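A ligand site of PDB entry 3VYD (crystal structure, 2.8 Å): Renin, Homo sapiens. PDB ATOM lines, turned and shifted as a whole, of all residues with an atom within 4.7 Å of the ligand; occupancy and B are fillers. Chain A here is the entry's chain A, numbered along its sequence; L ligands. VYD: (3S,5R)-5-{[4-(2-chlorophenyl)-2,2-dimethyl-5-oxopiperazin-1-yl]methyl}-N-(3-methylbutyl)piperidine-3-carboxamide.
The side-chain carboxylate (OD1) of Asp 38 is in salt-bridge range of a nitrogen (N25) of the ligand.
The side-chain hydroxyl of Thr 85 sits at hydrogen-bond distance from an oxygen (O29) of the ligand, at 2.7 Å.
N of Ser 84 lies within hydrogen-bond range of O30 of the ligand (2.7 Å).
A nitrogen (N25) of the ligand is in salt-bridge range of the side-chain carboxylate (OD2) of Asp 226 (2.8 Å).
A nitrogen (N28) of the ligand sits at hydrogen-bond distance from the backbone carbonyl oxygen (O) of Gly 40, 3.0 Å away.
The side-chain carboxylate of Asp 38 is in hydrogen-bond range of the backbone NH of Gly 40 (2.8 Å).
The backbone NH of Gly 228 sits close to the side-chain carboxylate of Asp 38.
OD2 of Asp 38 lies close to N of Ser 41.
The side-chain carboxylate of Asp 226 is in hydrogen-bond range of the backbone NH of Gly 228, 2.9 Å away.
O of Leu 121 lies within hydrogen-bond range of NE2 of Gln 19, at 3.0 Å.
Residues that only touch the ligand: Tyr 83 (3.2 Å), Gly 228 (3.4 Å), Gln 19 (3.4 Å), Phe 119 (3.4 Å), Arg 82 (3.5 Å), Pro 118 (3.6 Å), Ser 41 (3.7 Å), Ile 137 (3.7 Å), Phe 124 (3.8 Å) and Ala 229 (3.998 Å).
Hydrophobic or aromatic side chains that line the ligand: Tyr 83, Pro 118, Phe 119, Phe 124 and Ile 137.
Of the 21 residues printed, 15 come within 4 Å of the ligand.
Along chain A the residues within 4 Å of the ligand span positions 19 to 229.
The nearest printed residue that does not touch the ligand is Val 127 (4.1 Å).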
ATOM      1  N   THR A  18      -5.869  34.379  -8.536  1.00  0.00           N
ATOM      2  CA  THR A  18      -4.704  33.721  -7.978  1.00  0.00           C
ATOM      3  C   THR A  18      -3.929  32.830  -8.962  1.00  0.00           C
ATOM      4  O   THR A  18      -2.821  32.367  -8.672  1.00  0.00           O
ATOM      5  CB  THR A  18      -5.100  32.838  -6.816  1.00  0.00           C
ATOM      6  OG1 THR A  18      -5.935  31.782  -7.297  1.00  0.00           O
ATOM      7  CG2 THR A  18      -5.831  33.620  -5.776  1.00  0.00           C
ATOM      8  N   GLN A  19      -4.528  32.550 -10.112  1.00  0.00           N
ATOM      9  CA  GLN A  19      -3.873  31.707 -11.100  1.00  0.00           C
ATOM     10  C   GLN A  19      -4.153  32.264 -12.489  1.00  0.00           C
ATOM     11  O   GLN A  19      -5.328  32.436 -12.881  1.00  0.00           O
ATOM     12  CB  GLN A  19      -4.411  30.276 -11.032  1.00  0.00           C
ATOM     13  CG  GLN A  19      -4.134  29.589  -9.729  1.00  0.00           C
ATOM     14  CD  GLN A  19      -4.704  28.214  -9.672  1.00  0.00           C
ATOM     15  OE1 GLN A  19      -4.756  27.521 -10.680  1.00  0.00           O
ATOM     16  NE2 GLN A  19      -5.140  27.801  -8.483  1.00  0.00           N
ATOM     17  N   ASP A  38       5.911  31.509 -15.194  1.00  0.00           N
ATOM     18  CA  ASP A  38       6.566  31.871 -13.923  1.00  0.00           C
ATOM     19  C   ASP A  38       7.970  32.484 -14.088  1.00  0.00           C
ATOM     20  O   ASP A  38       8.944  31.755 -14.325  1.00  0.00           O
ATOM     21  CB  ASP A  38       6.670  30.649 -13.012  1.00  0.00           C
ATOM     22  CG  ASP A  38       7.381  30.951 -11.693  1.00  0.00           C
ATOM     23  OD1 ASP A  38       7.265  32.090 -11.174  1.00  0.00           O
ATOM     24  OD2 ASP A  38       8.035  30.032 -11.152  1.00  0.00           O
ATOM     25  N   GLY A  40       9.685  33.286 -11.848  1.00  0.00           N
ATOM     26  CA  GLY A  40      10.397  32.893 -10.645  1.00  0.00           C
ATOM     27  C   GLY A  40      11.033  31.532 -10.714  1.00  0.00           C
ATOM     28  O   GLY A  40      11.489  31.027  -9.701  1.00  0.00           O
ATOM     29  N   SER A  41      11.068  30.941 -11.899  1.00  0.00           N
ATOM     30  CA  SER A  41      11.667  29.618 -12.131  1.00  0.00           C
ATOM     31  C   SER A  41      11.965  29.541 -13.625  1.00  0.00           C
ATOM     32  O   SER A  41      11.579  30.425 -14.366  1.00  0.00           O
ATOM     33  CB  SER A  41      10.719  28.502 -11.675  1.00  0.00           C
ATOM     34  OG  SER A  41       9.435  28.552 -12.344  1.00  0.00           O
ATOM     35  N   ARG A  82      11.684  21.742  -6.932  1.00  0.00           N
ATOM     36  CA  ARG A  82      11.321  21.972  -5.545  1.00  0.00           C
ATOM     37  C   ARG A  82      11.009  23.408  -5.429  1.00  0.00           C
ATOM     38  O   ARG A  82      11.918  24.206  -5.235  1.00  0.00           O
ATOM     39  CB  ARG A  82      12.477  21.672  -4.609  1.00  0.00           C
ATOM     40  CG  ARG A  82      12.837  20.227  -4.533  1.00  0.00           C
ATOM     41  CD  ARG A  82      13.956  19.962  -3.563  1.00  0.00           C
ATOM     42  NE  ARG A  82      14.517  18.603  -3.723  1.00  0.00           N
ATOM     43  CZ  ARG A  82      15.258  18.173  -4.769  1.00  0.00           C
ATOM     44  NH1 ARG A  82      15.541  18.959  -5.806  1.00  0.00           N
ATOM     45  NH2 ARG A  82      15.704  16.939  -4.784  1.00  0.00           N
ATOM     46  N   TYR A  83       9.745  23.759  -5.548  1.00  0.00           N
ATOM     47  CA  TYR A  83       9.334  25.159  -5.453  1.00  0.00           C
ATOM     48  C   TYR A  83       9.033  25.510  -4.003  1.00  0.00           C
ATOM     49  O   TYR A  83       8.945  24.630  -3.158  1.00  0.00           O
ATOM     50  CB  TYR A  83       8.056  25.352  -6.233  1.00  0.00           C
ATOM     51  CG  TYR A  83       8.133  25.072  -7.705  1.00  0.00           C
ATOM     52  CD1 TYR A  83       7.269  24.143  -8.282  1.00  0.00           C
ATOM     53  CD2 TYR A  83       9.051  25.745  -8.534  1.00  0.00           C
ATOM     54  CE1 TYR A  83       7.275  23.892  -9.646  1.00  0.00           C
ATOM     55  CE2 TYR A  83       9.067  25.493  -9.915  1.00  0.00           C
ATOM     56  CZ  TYR A  83       8.176  24.557 -10.449  1.00  0.00           C
ATOM     57  OH  TYR A  83       8.153  24.260 -11.816  1.00  0.00           O
ATOM     58  N   SER A  84       8.808  26.800  -3.756  1.00  0.00           N
ATOM     59  CA  SER A  84       8.521  27.293  -2.411  1.00  0.00           C
ATOM     60  C   SER A  84       7.363  26.596  -1.734  1.00  0.00           C
ATOM     61  O   SER A  84       7.369  26.434  -0.533  1.00  0.00           O
ATOM     62  CB  SER A  84       8.296  28.799  -2.422  1.00  0.00           C
ATOM     63  OG  SER A  84       7.126  29.107  -3.158  1.00  0.00           O
ATOM     64  N   THR A  85       6.367  26.153  -2.479  1.00  0.00           N
ATOM     65  CA  THR A  85       5.202  25.618  -1.771  1.00  0.00           C
ATOM     66  C   THR A  85       4.784  24.200  -2.215  1.00  0.00           C
ATOM     67  O   THR A  85       3.623  23.794  -1.990  1.00  0.00           O
ATOM     68  CB  THR A  85       3.998  26.548  -1.962  1.00  0.00           C
ATOM     69  OG1 THR A  85       3.616  26.494  -3.337  1.00  0.00           O
ATOM     70  CG2 THR A  85       4.331  27.989  -1.548  1.00  0.00           C
ATOM     71  N   PRO A 118      -0.104  20.746  -3.385  1.00  0.00           N
ATOM     72  CA  PRO A 118      -1.208  21.625  -3.793  1.00  0.00           C
ATOM     73  C   PRO A 118      -1.828  21.382  -5.191  1.00  0.00           C
ATOM     74  O   PRO A 118      -2.807  22.000  -5.520  1.00  0.00           O
ATOM     75  CB  PRO A 118      -0.530  22.984  -3.797  1.00  0.00           C
ATOM     76  CG  PRO A 118       0.836  22.640  -4.375  1.00  0.00           C
ATOM     77  CD  PRO A 118       1.187  21.269  -3.855  1.00  0.00           C
ATOM     78  N   PHE A 119      -1.278  20.500  -5.994  1.00  0.00           N
ATOM     79  CA  PHE A 119      -1.614  20.490  -7.414  1.00  0.00           C
ATOM     80  C   PHE A 119      -3.054  20.173  -7.720  1.00  0.00           C
ATOM     81  O   PHE A 119      -3.567  20.404  -8.806  1.00  0.00           O
ATOM     82  CB  PHE A 119      -0.608  19.614  -8.192  1.00  0.00           C
ATOM     83  CG  PHE A 119       0.769  20.208  -8.162  1.00  0.00           C
ATOM     84  CD1 PHE A 119       1.057  21.341  -8.905  1.00  0.00           C
ATOM     85  CD2 PHE A 119       1.723  19.726  -7.287  1.00  0.00           C
ATOM     86  CE1 PHE A 119       2.296  21.943  -8.818  1.00  0.00           C
ATOM     87  CE2 PHE A 119       2.957  20.328  -7.191  1.00  0.00           C
ATOM     88  CZ  PHE A 119       3.243  21.442  -7.957  1.00  0.00           C
ATOM     89  N   LEU A 121      -5.248  21.688  -6.197  1.00  0.00           N
ATOM     90  CA  LEU A 121      -5.772  23.033  -6.084  1.00  0.00           C
ATOM     91  C   LEU A 121      -5.437  23.895  -7.305  1.00  0.00           C
ATOM     92  O   LEU A 121      -5.778  25.054  -7.327  1.00  0.00           O
ATOM     93  CB  LEU A 121      -5.215  23.711  -4.823  1.00  0.00           C
ATOM     94  CG  LEU A 121      -6.041  23.947  -3.546  1.00  0.00           C
ATOM     95  CD1 LEU A 121      -7.187  22.964  -3.355  1.00  0.00           C
ATOM     96  CD2 LEU A 121      -5.167  23.995  -2.288  1.00  0.00           C
ATOM     97  N   ALA A 122      -4.760  23.331  -8.298  1.00  0.00           N
ATOM     98  CA  ALA A 122      -4.394  24.077  -9.504  1.00  0.00           C
ATOM     99  C   ALA A 122      -5.404  23.894 -10.589  1.00  0.00           C
ATOM    100  O   ALA A 122      -5.753  22.777 -10.896  1.00  0.00           O
ATOM    101  CB  ALA A 122      -3.074  23.588 -10.041  1.00  0.00           C
ATOM    102  N   PHE A 124      -4.460  24.945 -13.697  1.00  0.00           N
ATOM    103  CA  PHE A 124      -3.550  24.644 -14.837  1.00  0.00           C
ATOM    104  C   PHE A 124      -3.035  23.216 -14.740  1.00  0.00           C
ATOM    105  O   PHE A 124      -3.326  22.534 -13.762  1.00  0.00           O
ATOM    106  CB  PHE A 124      -2.346  25.605 -14.818  1.00  0.00           C
ATOM    107  CG  PHE A 124      -1.612  25.611 -13.512  1.00  0.00           C
ATOM    108  CD1 PHE A 124      -2.046  26.412 -12.472  1.00  0.00           C
ATOM    109  CD2 PHE A 124      -0.496  24.774 -13.309  1.00  0.00           C
ATOM    110  CE1 PHE A 124      -1.363  26.407 -11.242  1.00  0.00           C
ATOM    111  CE2 PHE A 124       0.176  24.750 -12.084  1.00  0.00           C
ATOM    112  CZ  PHE A 124      -0.249  25.580 -11.052  1.00  0.00           C
ATOM    113  N   VAL A 127       3.754  24.208 -15.844  1.00  0.00           N
ATOM    114  CA  VAL A 127       4.441  25.494 -15.744  1.00  0.00           C
ATOM    115  C   VAL A 127       5.381  25.735 -16.915  1.00  0.00           C
ATOM    116  O   VAL A 127       5.991  24.819 -17.436  1.00  0.00           O
ATOM    117  CB  VAL A 127       5.208  25.626 -14.404  1.00  0.00           C
ATOM    118  CG1 VAL A 127       5.939  26.966 -14.305  1.00  0.00           C
ATOM    119  CG2 VAL A 127       4.247  25.408 -13.212  1.00  0.00           C
ATOM    120  N   GLN A 135      18.806  29.681 -13.129  1.00  0.00           N
ATOM    121  CA  GLN A 135      17.877  29.058 -12.170  1.00  0.00           C
ATOM    122  C   GLN A 135      17.255  27.719 -12.647  1.00  0.00           C
ATOM    123  O   GLN A 135      16.437  27.115 -11.926  1.00  0.00           O
ATOM    124  CB  GLN A 135      16.762  30.027 -11.835  1.00  0.00           C
ATOM    125  CG  GLN A 135      17.153  31.128 -10.897  1.00  0.00           C
ATOM    126  CD  GLN A 135      15.970  32.028 -10.621  1.00  0.00           C
ATOM    127  OE1 GLN A 135      15.355  32.574 -11.556  1.00  0.00           O
ATOM    128  NE2 GLN A 135      15.649  32.213  -9.357  1.00  0.00           N
ATOM    129  N   ILE A 137      16.840  23.972 -13.365  1.00  0.00           N
ATOM    130  CA  ILE A 137      17.336  22.731 -12.779  1.00  0.00           C
ATOM    131  C   ILE A 137      17.662  21.785 -13.931  1.00  0.00           C
ATOM    132  O   ILE A 137      16.969  21.799 -14.947  1.00  0.00           O
ATOM    133  CB  ILE A 137      16.354  22.134 -11.726  1.00  0.00           C
ATOM    134  CG1 ILE A 137      16.570  22.789 -10.374  1.00  0.00           C
ATOM    135  CG2 ILE A 137      16.531  20.643 -11.592  1.00  0.00           C
ATOM    136  CD1 ILE A 137      16.173  24.237 -10.309  1.00  0.00           C
ATOM    137  N   ASP A 226       7.715  38.379  -9.348  1.00  0.00           N
ATOM    138  CA  ASP A 226       7.309  36.966  -9.576  1.00  0.00           C
ATOM    139  C   ASP A 226       5.938  36.724 -10.172  1.00  0.00           C
ATOM    140  O   ASP A 226       4.922  36.734  -9.459  1.00  0.00           O
ATOM    141  CB  ASP A 226       7.386  36.216  -8.247  1.00  0.00           C
ATOM    142  CG  ASP A 226       7.356  34.728  -8.434  1.00  0.00           C
ATOM    143  OD1 ASP A 226       6.967  34.286  -9.541  1.00  0.00           O
ATOM    144  OD2 ASP A 226       7.732  34.023  -7.455  1.00  0.00           O
ATOM    145  N   GLY A 228       4.532  34.110 -11.132  1.00  0.00           N
ATOM    146  CA  GLY A 228       4.010  32.765 -10.874  1.00  0.00           C
ATOM    147  C   GLY A 228       3.474  32.716  -9.466  1.00  0.00           C
ATOM    148  O   GLY A 228       2.978  31.678  -9.038  1.00  0.00           O
ATOM    149  N   ALA A 229       3.580  33.831  -8.756  1.00  0.00           N
ATOM    150  CA  ALA A 229       3.112  33.924  -7.387  1.00  0.00           C
ATOM    151  C   ALA A 229       1.796  34.704  -7.332  1.00  0.00           C
ATOM    152  O   ALA A 229       1.659  35.774  -7.950  1.00  0.00           O
ATOM    153  CB  ALA A 229       4.178  34.557  -6.496  1.00  0.00           C
ATOM    154  N   SER A 230       0.837  34.180  -6.572  1.00  0.00           N
ATOM    155  CA  SER A 230      -0.456  34.803  -6.377  1.00  0.00           C
ATOM    156  C   SER A 230      -0.376  36.040  -5.516  1.00  0.00           C
ATOM    157  O   SER A 230      -1.122  36.987  -5.741  1.00  0.00           O
ATOM    158  CB  SER A 230      -1.410  33.825  -5.701  1.00  0.00           C
ATOM    159  OG  SER A 230      -1.440  32.598  -6.370  1.00  0.00           O
HETATM  160  C1  VYD L   1      -1.377  28.450  -7.046  1.00  0.00           C
HETATM  161  C2  VYD L   1      -2.166  27.326  -6.914  1.00  0.00           C
HETATM  162  C3  VYD L   1      -0.017  28.323  -7.304  1.00  0.00           C
HETATM  163  C4  VYD L   1      -1.641  26.053  -7.031  1.00  0.00           C
HETATM  164  C5  VYD L   1       0.529  27.077  -7.410  1.00  0.00           C
HETATM  165  C6  VYD L   1      -0.281  25.966  -7.280  1.00  0.00           C
HETATM  166  C7  VYD L   1       2.744  26.681  -6.634  1.00  0.00           C
HETATM  167  C8  VYD L   1       9.689  28.862  -7.014  1.00  0.00           C
HETATM  168  C9  VYD L   1       3.860  27.634  -6.549  1.00  0.00           C
HETATM  169  C10 VYD L   1       7.311  28.809  -7.415  1.00  0.00           C
HETATM  170  C11 VYD L   1       8.675  30.895  -7.713  1.00  0.00           C
HETATM  171  C12 VYD L   1       6.345  31.036  -8.029  1.00  0.00           C
HETATM  172  C13 VYD L   1       2.336  27.744  -8.761  1.00  0.00           C
HETATM  173  C14 VYD L   1       8.628  29.399  -7.874  1.00  0.00           C
HETATM  174  C15 VYD L   1       6.224  29.530  -8.187  1.00  0.00           C
HETATM  175  C16 VYD L   1       3.772  27.394  -8.948  1.00  0.00           C
HETATM  176  C17 VYD L   1       4.150  28.189 -10.161  1.00  0.00           C
HETATM  177  C18 VYD L   1       3.990  25.912  -9.174  1.00  0.00           C
HETATM  178  C19 VYD L   1      13.001  25.558  -8.851  1.00  0.00           C
HETATM  179  C20 VYD L   1      13.391  28.034  -9.192  1.00  0.00           C
HETATM  180  C21 VYD L   1       4.831  29.164  -7.741  1.00  0.00           C
HETATM  181  C22 VYD L   1      12.249  27.190  -7.112  1.00  0.00           C
HETATM  182  C23 VYD L   1      12.107  28.650  -6.862  1.00  0.00           C
HETATM  183  C24 VYD L   1      13.288  26.900  -8.189  1.00  0.00           C
HETATM  184  N25 VYD L   1       7.633  31.479  -8.554  1.00  0.00           N
HETATM  185  N26 VYD L   1       1.879  26.942  -7.674  1.00  0.00           N
HETATM  186  N27 VYD L   1       4.595  27.733  -7.786  1.00  0.00           N
HETATM  187  N28 VYD L   1      10.923  29.021  -7.598  1.00  0.00           N
HETATM  188  O29 VYD L   1       2.704  25.805  -5.808  1.00  0.00           O
HETATM  189  O30 VYD L   1       9.456  28.351  -5.931  1.00  0.00           O
HETATM  190 CL   VYD L   1       0.434  24.444  -7.443  1.00  0.00          CL
